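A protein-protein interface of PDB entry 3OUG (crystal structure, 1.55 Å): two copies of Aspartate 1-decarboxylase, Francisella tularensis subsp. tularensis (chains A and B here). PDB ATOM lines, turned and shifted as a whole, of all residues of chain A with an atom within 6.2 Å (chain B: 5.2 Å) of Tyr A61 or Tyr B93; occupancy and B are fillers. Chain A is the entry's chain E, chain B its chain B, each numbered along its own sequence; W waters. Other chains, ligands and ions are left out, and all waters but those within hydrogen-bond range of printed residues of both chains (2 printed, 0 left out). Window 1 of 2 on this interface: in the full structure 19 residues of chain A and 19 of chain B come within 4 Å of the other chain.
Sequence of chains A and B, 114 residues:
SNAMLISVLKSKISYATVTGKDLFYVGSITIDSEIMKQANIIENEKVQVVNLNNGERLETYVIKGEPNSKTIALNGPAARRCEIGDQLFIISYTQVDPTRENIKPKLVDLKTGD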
ATOM      1  N   TYR A  25     -26.605   4.687  -8.428  1.00  0.00           N
ATOM      2  CA  TYR A  25     -26.709   4.750  -6.961  1.00  0.00           C
ATOM      3  C   TYR A  25     -27.106   6.143  -6.466  1.00  0.00           C
ATOM      4  O   TYR A  25     -27.869   6.276  -5.487  1.00  0.00           O
ATOM      5  CB  TYR A  25     -25.362   4.342  -6.349  1.00  0.00           C
ATOM      6  CG  TYR A  25     -25.364   4.253  -4.857  1.00  0.00           C
ATOM      7  CD1 TYR A  25     -26.045   3.232  -4.209  1.00  0.00           C
ATOM      8  CD2 TYR A  25     -24.700   5.200  -4.079  1.00  0.00           C
ATOM      9  CE1 TYR A  25     -26.076   3.150  -2.834  1.00  0.00           C
ATOM     10  CE2 TYR A  25     -24.732   5.129  -2.709  1.00  0.00           C
ATOM     11  CZ  TYR A  25     -25.423   4.095  -2.093  1.00  0.00           C
ATOM     12  OH  TYR A  25     -25.458   4.016  -0.726  1.00  0.00           O
ATOM     13  N   SER A  28     -19.553   2.672  -5.242  1.00  0.00           N
ATOM     14  CA  SER A  28     -19.005   2.249  -3.948  1.00  0.00           C
ATOM     15  C   SER A  28     -19.258   0.756  -3.812  1.00  0.00           C
ATOM     16  O   SER A  28     -19.847   0.149  -4.735  1.00  0.00           O
ATOM     17  CB  SER A  28     -19.696   3.001  -2.842  1.00  0.00           C
ATOM     18  N   ILE A  29     -18.801   0.158  -2.726  1.00  0.00           N
ATOM     19  CA  ILE A  29     -19.110  -1.258  -2.449  1.00  0.00           C
ATOM     20  C   ILE A  29     -19.908  -1.341  -1.155  1.00  0.00           C
ATOM     21  O   ILE A  29     -19.479  -0.821  -0.115  1.00  0.00           O
ATOM     22  CB  ILE A  29     -17.835  -2.165  -2.405  1.00  0.00           C
ATOM     23  CG1 ILE A  29     -18.278  -3.622  -2.247  1.00  0.00           C
ATOM     24  CG2 ILE A  29     -16.847  -1.757  -1.313  1.00  0.00           C
ATOM     25  CD1 ILE A  29     -17.153  -4.632  -2.445  1.00  0.00           C
ATOM     26  N   THR A  30     -21.061  -1.989  -1.227  1.00  0.00           N
ATOM     27  CA  THR A  30     -21.874  -2.206  -0.046  1.00  0.00           C
ATOM     28  C   THR A  30     -21.519  -3.580   0.503  1.00  0.00           C
ATOM     29  O   THR A  30     -21.568  -4.564  -0.241  1.00  0.00           O
ATOM     30  CB  THR A  30     -23.352  -2.170  -0.412  1.00  0.00           C
ATOM     31  OG1 THR A  30     -23.686  -0.871  -0.903  1.00  0.00           O
ATOM     32  CG2 THR A  30     -24.227  -2.456   0.830  1.00  0.00           C
ATOM     33  N   ASN A  44     -17.044   4.036   4.997  1.00  0.00           N
ATOM     34  CA  ASN A  44     -16.309   5.050   4.238  1.00  0.00           C
ATOM     35  C   ASN A  44     -14.826   4.815   4.078  1.00  0.00           C
ATOM     36  O   ASN A  44     -14.163   5.637   3.475  1.00  0.00           O
ATOM     37  CB  ASN A  44     -16.557   6.478   4.760  1.00  0.00           C
ATOM     38  CG  ASN A  44     -18.002   6.866   4.690  1.00  0.00           C
ATOM     39  OD1 ASN A  44     -18.654   6.715   3.654  1.00  0.00           O
ATOM     40  ND2 ASN A  44     -18.533   7.365   5.809  1.00  0.00           N
ATOM     41  N   GLU A  45     -14.329   3.672   4.530  1.00  0.00           N
ATOM     42  CA  GLU A  45     -12.942   3.318   4.367  1.00  0.00           C
ATOM     43  C   GLU A  45     -12.663   2.972   2.900  1.00  0.00           C
ATOM     44  O   GLU A  45     -13.489   2.345   2.240  1.00  0.00           O
ATOM     45  CB  GLU A  45     -12.583   2.142   5.262  1.00  0.00           C
ATOM     46  CG  GLU A  45     -11.145   1.743   5.202  1.00  0.00           C
ATOM     47  CD  GLU A  45     -10.702   0.834   6.343  1.00  0.00           C
ATOM     48  OE1 GLU A  45     -11.492   0.565   7.292  1.00  0.00           O
ATOM     49  OE2 GLU A  45      -9.543   0.366   6.281  1.00  0.00           O
ATOM     50  N   LYS A  46     -11.500   3.381   2.427  1.00  0.00           N
ATOM     51  CA  LYS A  46     -11.030   3.040   1.081  1.00  0.00           C
ATOM     52  C   LYS A  46     -10.574   1.581   1.046  1.00  0.00           C
ATOM     53  O   LYS A  46      -9.806   1.127   1.911  1.00  0.00           O
ATOM     54  CB  LYS A  46      -9.898   3.974   0.673  1.00  0.00           C
ATOM     55  CG  LYS A  46      -9.392   3.801  -0.752  1.00  0.00           C
ATOM     56  CD  LYS A  46      -8.242   4.756  -1.007  1.00  0.00           C
ATOM     57  CE  LYS A  46      -7.766   4.748  -2.453  1.00  0.00           C
ATOM     58  NZ  LYS A  46      -6.451   5.457  -2.563  1.00  0.00           N
ATOM     59  N   VAL A  47     -11.012   0.857   0.014  1.00  0.00           N
ATOM     60  CA  VAL A  47     -10.606  -0.539  -0.154  1.00  0.00           C
ATOM     61  C   VAL A  47     -10.275  -0.822  -1.608  1.00  0.00           C
ATOM     62  O   VAL A  47     -10.796  -0.157  -2.498  1.00  0.00           O
ATOM     63  CB  VAL A  47     -11.696  -1.545   0.290  1.00  0.00           C
ATOM     64  CG1 VAL A  47     -11.836  -1.507   1.821  1.00  0.00           C
ATOM     65  CG2 VAL A  47     -13.000  -1.265  -0.376  1.00  0.00           C
ATOM     66  N   GLU A  59     -10.347   0.635  -6.833  1.00  0.00           N
ATOM     67  CA  GLU A  59     -10.390   1.162  -5.481  1.00  0.00           C
ATOM     68  C   GLU A  59     -11.680   1.954  -5.337  1.00  0.00           C
ATOM     69  O   GLU A  59     -12.094   2.698  -6.248  1.00  0.00           O
ATOM     70  CB  GLU A  59      -9.179   2.069  -5.219  1.00  0.00           C
ATOM     71  CG  GLU A  59      -7.860   1.298  -5.140  1.00  0.00           C
ATOM     72  CD  GLU A  59      -6.627   2.188  -4.932  1.00  0.00           C
ATOM     73  OE1 GLU A  59      -6.546   3.284  -5.551  1.00  0.00           O
ATOM     74  OE2 GLU A  59      -5.740   1.789  -4.138  1.00  0.00           O
ATOM     75  N   THR A  60     -12.332   1.788  -4.186  1.00  0.00           N
ATOM     76  CA  THR A  60     -13.563   2.521  -3.911  1.00  0.00           C
ATOM     77  C   THR A  60     -13.725   2.586  -2.382  1.00  0.00           C
ATOM     78  O   THR A  60     -12.825   2.207  -1.674  1.00  0.00           O
ATOM     79  CB  THR A  60     -14.779   1.916  -4.640  1.00  0.00           C
ATOM     80  OG1 THR A  60     -15.886   2.832  -4.542  1.00  0.00           O
ATOM     81  CG2 THR A  60     -15.136   0.551  -4.064  1.00  0.00           C
ATOM     82  N   TYR A  61     -14.850   3.088  -1.900  1.00  0.00           N
ATOM     83  CA  TYR A  61     -15.085   3.193  -0.458  1.00  0.00           C
ATOM     84  C   TYR A  61     -16.242   2.277  -0.057  1.00  0.00           C
ATOM     85  O   TYR A  61     -17.028   1.861  -0.900  1.00  0.00           O
ATOM     86  CB  TYR A  61     -15.337   4.665  -0.068  1.00  0.00           C
ATOM     87  CG  TYR A  61     -16.624   5.238  -0.562  1.00  0.00           C
ATOM     88  CD1 TYR A  61     -16.712   5.825  -1.816  1.00  0.00           C
ATOM     89  CD2 TYR A  61     -17.780   5.181   0.220  1.00  0.00           C
ATOM     90  CE1 TYR A  61     -17.902   6.343  -2.286  1.00  0.00           C
ATOM     91  CE2 TYR A  61     -18.977   5.705  -0.236  1.00  0.00           C
ATOM     92  CZ  TYR A  61     -19.041   6.278  -1.491  1.00  0.00           C
ATOM     93  OH  TYR A  61     -20.232   6.795  -1.953  1.00  0.00           O
ATOM     94  N   VAL A  62     -16.328   1.988   1.246  1.00  0.00           N
ATOM     95  CA  VAL A  62     -17.304   1.015   1.760  1.00  0.00           C
ATOM     96  C   VAL A  62     -18.573   1.679   2.276  1.00  0.00           C
ATOM     97  O   VAL A  62     -18.513   2.679   2.992  1.00  0.00           O
ATOM     98  CB  VAL A  62     -16.706   0.191   2.903  1.00  0.00           C
ATOM     99  CG1 VAL A  62     -17.783  -0.750   3.497  1.00  0.00           C
ATOM    100  CG2 VAL A  62     -15.489  -0.608   2.408  1.00  0.00           C
ATOM    101  N   ILE A  63     -19.707   1.095   1.916  1.00  0.00           N
ATOM    102  CA  ILE A  63     -21.026   1.456   2.446  1.00  0.00           C
ATOM    103  C   ILE A  63     -21.582   0.276   3.236  1.00  0.00           C
ATOM    104  O   ILE A  63     -21.396  -0.871   2.864  1.00  0.00           O
ATOM    105  CB  ILE A  63     -21.989   1.825   1.306  1.00  0.00           C
ATOM    106  CG1 ILE A  63     -21.492   3.079   0.581  1.00  0.00           C
ATOM    107  CG2 ILE A  63     -23.389   2.066   1.842  1.00  0.00           C
ATOM    108  CD1 ILE A  63     -22.202   3.319  -0.734  1.00  0.00           C
ATOM    109  N   SER B   7      -7.001   5.312   4.844  1.00  0.00           N
ATOM    110  CA  SER B   7      -7.670   6.259   3.962  1.00  0.00           C
ATOM    111  C   SER B   7      -9.184   6.098   4.090  1.00  0.00           C
ATOM    112  O   SER B   7      -9.713   4.958   4.088  1.00  0.00           O
ATOM    113  CB  SER B   7      -7.231   6.037   2.518  1.00  0.00           C
ATOM    114  OG  SER B   7      -5.868   6.379   2.368  1.00  0.00           O
ATOM    115  N   VAL B   8      -9.866   7.237   4.236  1.00  0.00           N
ATOM    116  CA  VAL B   8     -11.320   7.295   4.339  1.00  0.00           C
ATOM    117  C   VAL B   8     -11.875   8.388   3.419  1.00  0.00           C
ATOM    118  O   VAL B   8     -11.160   9.323   3.055  1.00  0.00           O
ATOM    119  CB  VAL B   8     -11.812   7.525   5.768  1.00  0.00           C
ATOM    120  CG1 VAL B   8     -11.317   6.412   6.698  1.00  0.00           C
ATOM    121  CG2 VAL B   8     -11.401   8.896   6.270  1.00  0.00           C
ATOM    122  N   LEU B   9     -13.140   8.232   3.032  1.00  0.00           N
ATOM    123  CA  LEU B   9     -13.821   9.204   2.181  1.00  0.00           C
ATOM    124  C   LEU B   9     -13.961  10.526   2.896  1.00  0.00           C
ATOM    125  O   LEU B   9     -14.454  10.564   4.044  1.00  0.00           O
ATOM    126  CB  LEU B   9     -15.208   8.691   1.798  1.00  0.00           C
ATOM    127  CG  LEU B   9     -16.006   9.527   0.788  1.00  0.00           C
ATOM    128  CD1 LEU B   9     -15.347   9.580  -0.596  1.00  0.00           C
ATOM    129  CD2 LEU B   9     -17.452   8.973   0.751  1.00  0.00           C
ATOM    130  N   LYS B  10     -13.562  11.606   2.229  1.00  0.00           N
ATOM    131  CA  LYS B  10     -13.712  12.962   2.777  1.00  0.00           C
ATOM    132  C   LYS B  10     -14.798  13.766   2.065  1.00  0.00           C
ATOM    133  O   LYS B  10     -15.535  14.513   2.699  1.00  0.00           O
ATOM    134  CB  LYS B  10     -12.379  13.695   2.636  1.00  0.00           C
ATOM    135  CG  LYS B  10     -12.361  15.172   3.039  1.00  0.00           C
ATOM    136  CD  LYS B  10     -11.025  15.772   2.590  1.00  0.00           C
ATOM    137  CE  LYS B  10     -11.199  17.064   1.820  1.00  0.00           C
ATOM    138  NZ  LYS B  10     -11.746  16.892   0.445  1.00  0.00           N
ATOM    139  N   LYS B  12     -17.520  13.742  -1.679  1.00  0.00           N
ATOM    140  CA  LYS B  12     -18.034  13.114  -2.898  1.00  0.00           C
ATOM    141  C   LYS B  12     -19.018  14.026  -3.603  1.00  0.00           C
ATOM    142  O   LYS B  12     -19.987  14.517  -3.002  1.00  0.00           O
ATOM    143  CB  LYS B  12     -18.705  11.778  -2.585  1.00  0.00           C
ATOM    144  CG  LYS B  12     -19.074  10.972  -3.836  1.00  0.00           C
ATOM    145  CD  LYS B  12     -19.678   9.628  -3.480  1.00  0.00           C
ATOM    146  CE  LYS B  12     -19.786   8.708  -4.684  1.00  0.00           C
ATOM    147  NZ  LYS B  12     -20.727   7.541  -4.419  1.00  0.00           N
ATOM    148  N   GLU B  45      -6.267  19.787  -5.278  1.00  0.00           N
ATOM    149  CA  GLU B  45      -6.460  18.567  -4.498  1.00  0.00           C
ATOM    150  C   GLU B  45      -6.557  17.358  -5.452  1.00  0.00           C
ATOM    151  O   GLU B  45      -7.125  17.477  -6.518  1.00  0.00           O
ATOM    152  CB  GLU B  45      -7.735  18.642  -3.652  1.00  0.00           C
ATOM    153  CG  GLU B  45      -7.892  17.483  -2.700  1.00  0.00           C
ATOM    154  CD  GLU B  45      -8.980  17.700  -1.644  1.00  0.00           C
ATOM    155  OE1 GLU B  45      -9.439  18.857  -1.442  1.00  0.00           O
ATOM    156  OE2 GLU B  45      -9.373  16.693  -1.008  1.00  0.00           O
ATOM    157  N   LYS B  46      -5.993  16.230  -5.048  1.00  0.00           N
ATOM    158  CA  LYS B  46      -6.138  14.966  -5.811  1.00  0.00           C
ATOM    159  C   LYS B  46      -7.532  14.375  -5.627  1.00  0.00           C
ATOM    160  O   LYS B  46      -8.062  14.304  -4.492  1.00  0.00           O
ATOM    161  CB  LYS B  46      -5.077  13.973  -5.359  1.00  0.00           C
ATOM    162  CG  LYS B  46      -4.940  12.692  -6.224  1.00  0.00           C
ATOM    163  CD  LYS B  46      -3.991  11.726  -5.531  1.00  0.00           C
ATOM    164  CE  LYS B  46      -3.910  10.388  -6.243  1.00  0.00           C
ATOM    165  NZ  LYS B  46      -3.015   9.436  -5.495  1.00  0.00           N
ATOM    166  N   GLN B  48     -10.345  11.181  -7.181  1.00  0.00           N
ATOM    167  CA  GLN B  48     -10.716  10.069  -8.069  1.00  0.00           C
ATOM    168  C   GLN B  48     -11.936  10.474  -8.871  1.00  0.00           C
ATOM    169  O   GLN B  48     -12.912  10.985  -8.329  1.00  0.00           O
ATOM    170  CB  GLN B  48     -11.010   8.845  -7.217  1.00  0.00           C
ATOM    171  CG  GLN B  48     -11.382   7.605  -7.998  1.00  0.00           C
ATOM    172  CD  GLN B  48     -11.784   6.451  -7.105  1.00  0.00           C
ATOM    173  OE1 GLN B  48     -12.555   6.625  -6.155  1.00  0.00           O
ATOM    174  NE2 GLN B  48     -11.306   5.240  -7.438  1.00  0.00           N
ATOM    175  N   ILE B  91     -14.498  12.063  -6.187  1.00  0.00           N
ATOM    176  CA  ILE B  91     -14.250  11.575  -4.828  1.00  0.00           C
ATOM    177  C   ILE B  91     -12.891  12.033  -4.286  1.00  0.00           C
ATOM    178  O   ILE B  91     -11.880  11.955  -4.955  1.00  0.00           O
ATOM    179  CB  ILE B  91     -14.294  10.029  -4.833  1.00  0.00           C
ATOM    180  CG1 ILE B  91     -15.716   9.550  -5.134  1.00  0.00           C
ATOM    181  CG2 ILE B  91     -13.831   9.467  -3.477  1.00  0.00           C
ATOM    182  CD1 ILE B  91     -15.814   8.085  -5.489  1.00  0.00           C
ATOM    183  N   SER B  92     -12.858  12.507  -3.039  1.00  0.00           N
ATOM    184  CA  SER B  92     -11.565  12.761  -2.377  1.00  0.00           C
ATOM    185  C   SER B  92     -11.488  12.008  -1.063  1.00  0.00           C
ATOM    186  O   SER B  92     -12.501  11.806  -0.402  1.00  0.00           O
ATOM    187  CB  SER B  92     -11.297  14.246  -2.147  1.00  0.00           C
ATOM    188  OG  SER B  92     -11.991  14.758  -1.025  1.00  0.00           O
ATOM    189  N   TYR B  93     -10.287  11.534  -0.754  1.00  0.00           N
ATOM    190  CA  TYR B  93     -10.028  10.735   0.432  1.00  0.00           C
ATOM    191  C   TYR B  93      -9.092  11.529   1.340  1.00  0.00           C
ATOM    192  O   TYR B  93      -8.449  12.492   0.905  1.00  0.00           O
ATOM    193  CB  TYR B  93      -9.347   9.424   0.056  1.00  0.00           C
ATOM    194  CG  TYR B  93     -10.199   8.497  -0.798  1.00  0.00           C
ATOM    195  CD1 TYR B  93     -11.132   7.647  -0.219  1.00  0.00           C
ATOM    196  CD2 TYR B  93     -10.074   8.486  -2.177  1.00  0.00           C
ATOM    197  CE1 TYR B  93     -11.900   6.780  -1.009  1.00  0.00           C
ATOM    198  CE2 TYR B  93     -10.843   7.615  -2.975  1.00  0.00           C
ATOM    199  CZ  TYR B  93     -11.755   6.782  -2.374  1.00  0.00           C
ATOM    200  OH  TYR B  93     -12.541   5.925  -3.142  1.00  0.00           O
ATOM    201  N   THR B  94      -9.021  11.095   2.592  1.00  0.00           N
ATOM    202  CA  THR B  94      -8.127  11.675   3.578  1.00  0.00           C
ATOM    203  C   THR B  94      -7.530  10.538   4.401  1.00  0.00           C
ATOM    204  O   THR B  94      -8.193   9.525   4.630  1.00  0.00           O
ATOM    205  CB  THR B  94      -8.879  12.686   4.466  1.00  0.00           C
ATOM    206  OG1 THR B  94      -7.969  13.286   5.395  1.00  0.00           O
ATOM    207  CG2 THR B  94     -10.022  12.033   5.235  1.00  0.00           C
ATOM    208  N   GLN B  95      -6.268  10.686   4.792  1.00  0.00           N
ATOM    209  CA  GLN B  95      -5.585   9.734   5.662  1.00  0.00           C
ATOM    210  C   GLN B  95      -5.762  10.163   7.103  1.00  0.00           C
ATOM    211  O   GLN B  95      -5.473  11.307   7.434  1.00  0.00           O
ATOM    212  CB  GLN B  95      -4.098   9.693   5.360  1.00  0.00           C
ATOM    213  CG  GLN B  95      -3.718   9.002   4.072  1.00  0.00           C
ATOM    214  CD  GLN B  95      -2.708   7.895   4.325  1.00  0.00           C
ATOM    215  OE1 GLN B  95      -1.482   8.075   4.185  1.00  0.00           O
ATOM    216  NE2 GLN B  95      -3.230   6.728   4.728  1.00  0.00           N
HETATM  217  O   HOH W   1     -15.332   5.107  -6.033  1.00  0.00           O
HETATM  218  O   HOH W   2      -7.712   2.468   4.131  1.00  0.00           O
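Water W1 lies within hydrogen-bond range of OG1 of Thr A60 (2.8 Å) and OE1 of Gln B48 (3.2 Å).
Water W2 bridges N of Ser B7 (3.0 Å) and O of Lys A46 (3.3 Å).
Of the printed residues of chain B, Glu A45 touches Ser B7.
Of the printed residues of chain B, Glu A59 touches Gln B48.
Of chain B, only Leu B9 (3.7 Å), Lys B12 (2.6 Å) and Tyr B93 (3.9 Å) come within 4 Å of Tyr A61.
Lys B10 touches none of the printed residues of chain A.
Of the printed residues of chain A, Lys B12 touches Tyr A61 (2.6 Å).
Of the printed residues of chain A, Gln B48 touches Glu A59.
Of chain A, only Lys A46, Thr A60 and Tyr A61 come within 4 Å of Tyr B93.
O of Ser B7 sits at hydrogen-bond distance from N of Lys A46, at 2.9 Å.
The backbone NH (N) of Leu B9 sits at hydrogen-bond distance from the backbone carbonyl oxygen (O) of Asn A44 (2.8 Å).
The side-chain hydroxyl (OH) of Tyr A61 lies within hydrogen-bond range of the side-chain amino group (NZ) of Lys B12 (2.6 Å).
The backbone carbonyl oxygen (O) of Glu A59 sits at hydrogen-bond distance from the side-chain amide nitrogen (NE2) of Gln B48 (2.9 Å).
Hydrophobic or aromatic side chains of chain A that line the printed part of chain B: Tyr A61.
Of the 13 printed residues of chain B, 6 touch a printed residue of chain A.
Among the printed residues, 10 pairs touch across the chains.
Among the printed residues, no Asp or Glu carboxylate lies within 4 Å of a Lys or Arg side-chain nitrogen of the other chain.
The backbone NH (N) of Gln B48 is in hydrogen-bond range of the backbone carbonyl oxygen (O) of Ile B91 (2.8 Å).
The side-chain amide oxygen (OE1) of Gln B48 lies within hydrogen-bond range of the side-chain hydroxyl (OH) of Tyr B93 (3.1 Å).
O of Tyr A61 sits at hydrogen-bond distance from N of Ile A29 (3.1 Å).
The backbone carbonyl oxygen (O) of Val A62 is in hydrogen-bond range of the backbone NH (N) of Asn A44.
The backbone carbonyl oxygen of Glu A45 sits at hydrogen-bond distance from the backbone NH of Val A62, at 3.0 Å.
The backbone carbonyl oxygen (O) of Thr A60 lies within hydrogen-bond range of the backbone NH (N) of Val A47 (2.8 Å).
O of Asn A44 touches CA of Val B8 (3.4 Å).
CA of Glu A45 touches O of Ser B7 (3.6 Å).
CB of Lys A46 touches CE1 of Tyr B93, at 3.8 Å.
Thr A60 touches Tyr B93.
Leu B9 touches Tyr A61 (CD2 to CE2, 3.7 Å).
Tyr B93 touches Tyr A61 (OH to N, 3.9 Å).
Positions printed for both chains: 45 and 46.
Of the 10 pairs that touch across the chains among the printed residues, none has its exchanged pair printed and touching as well.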
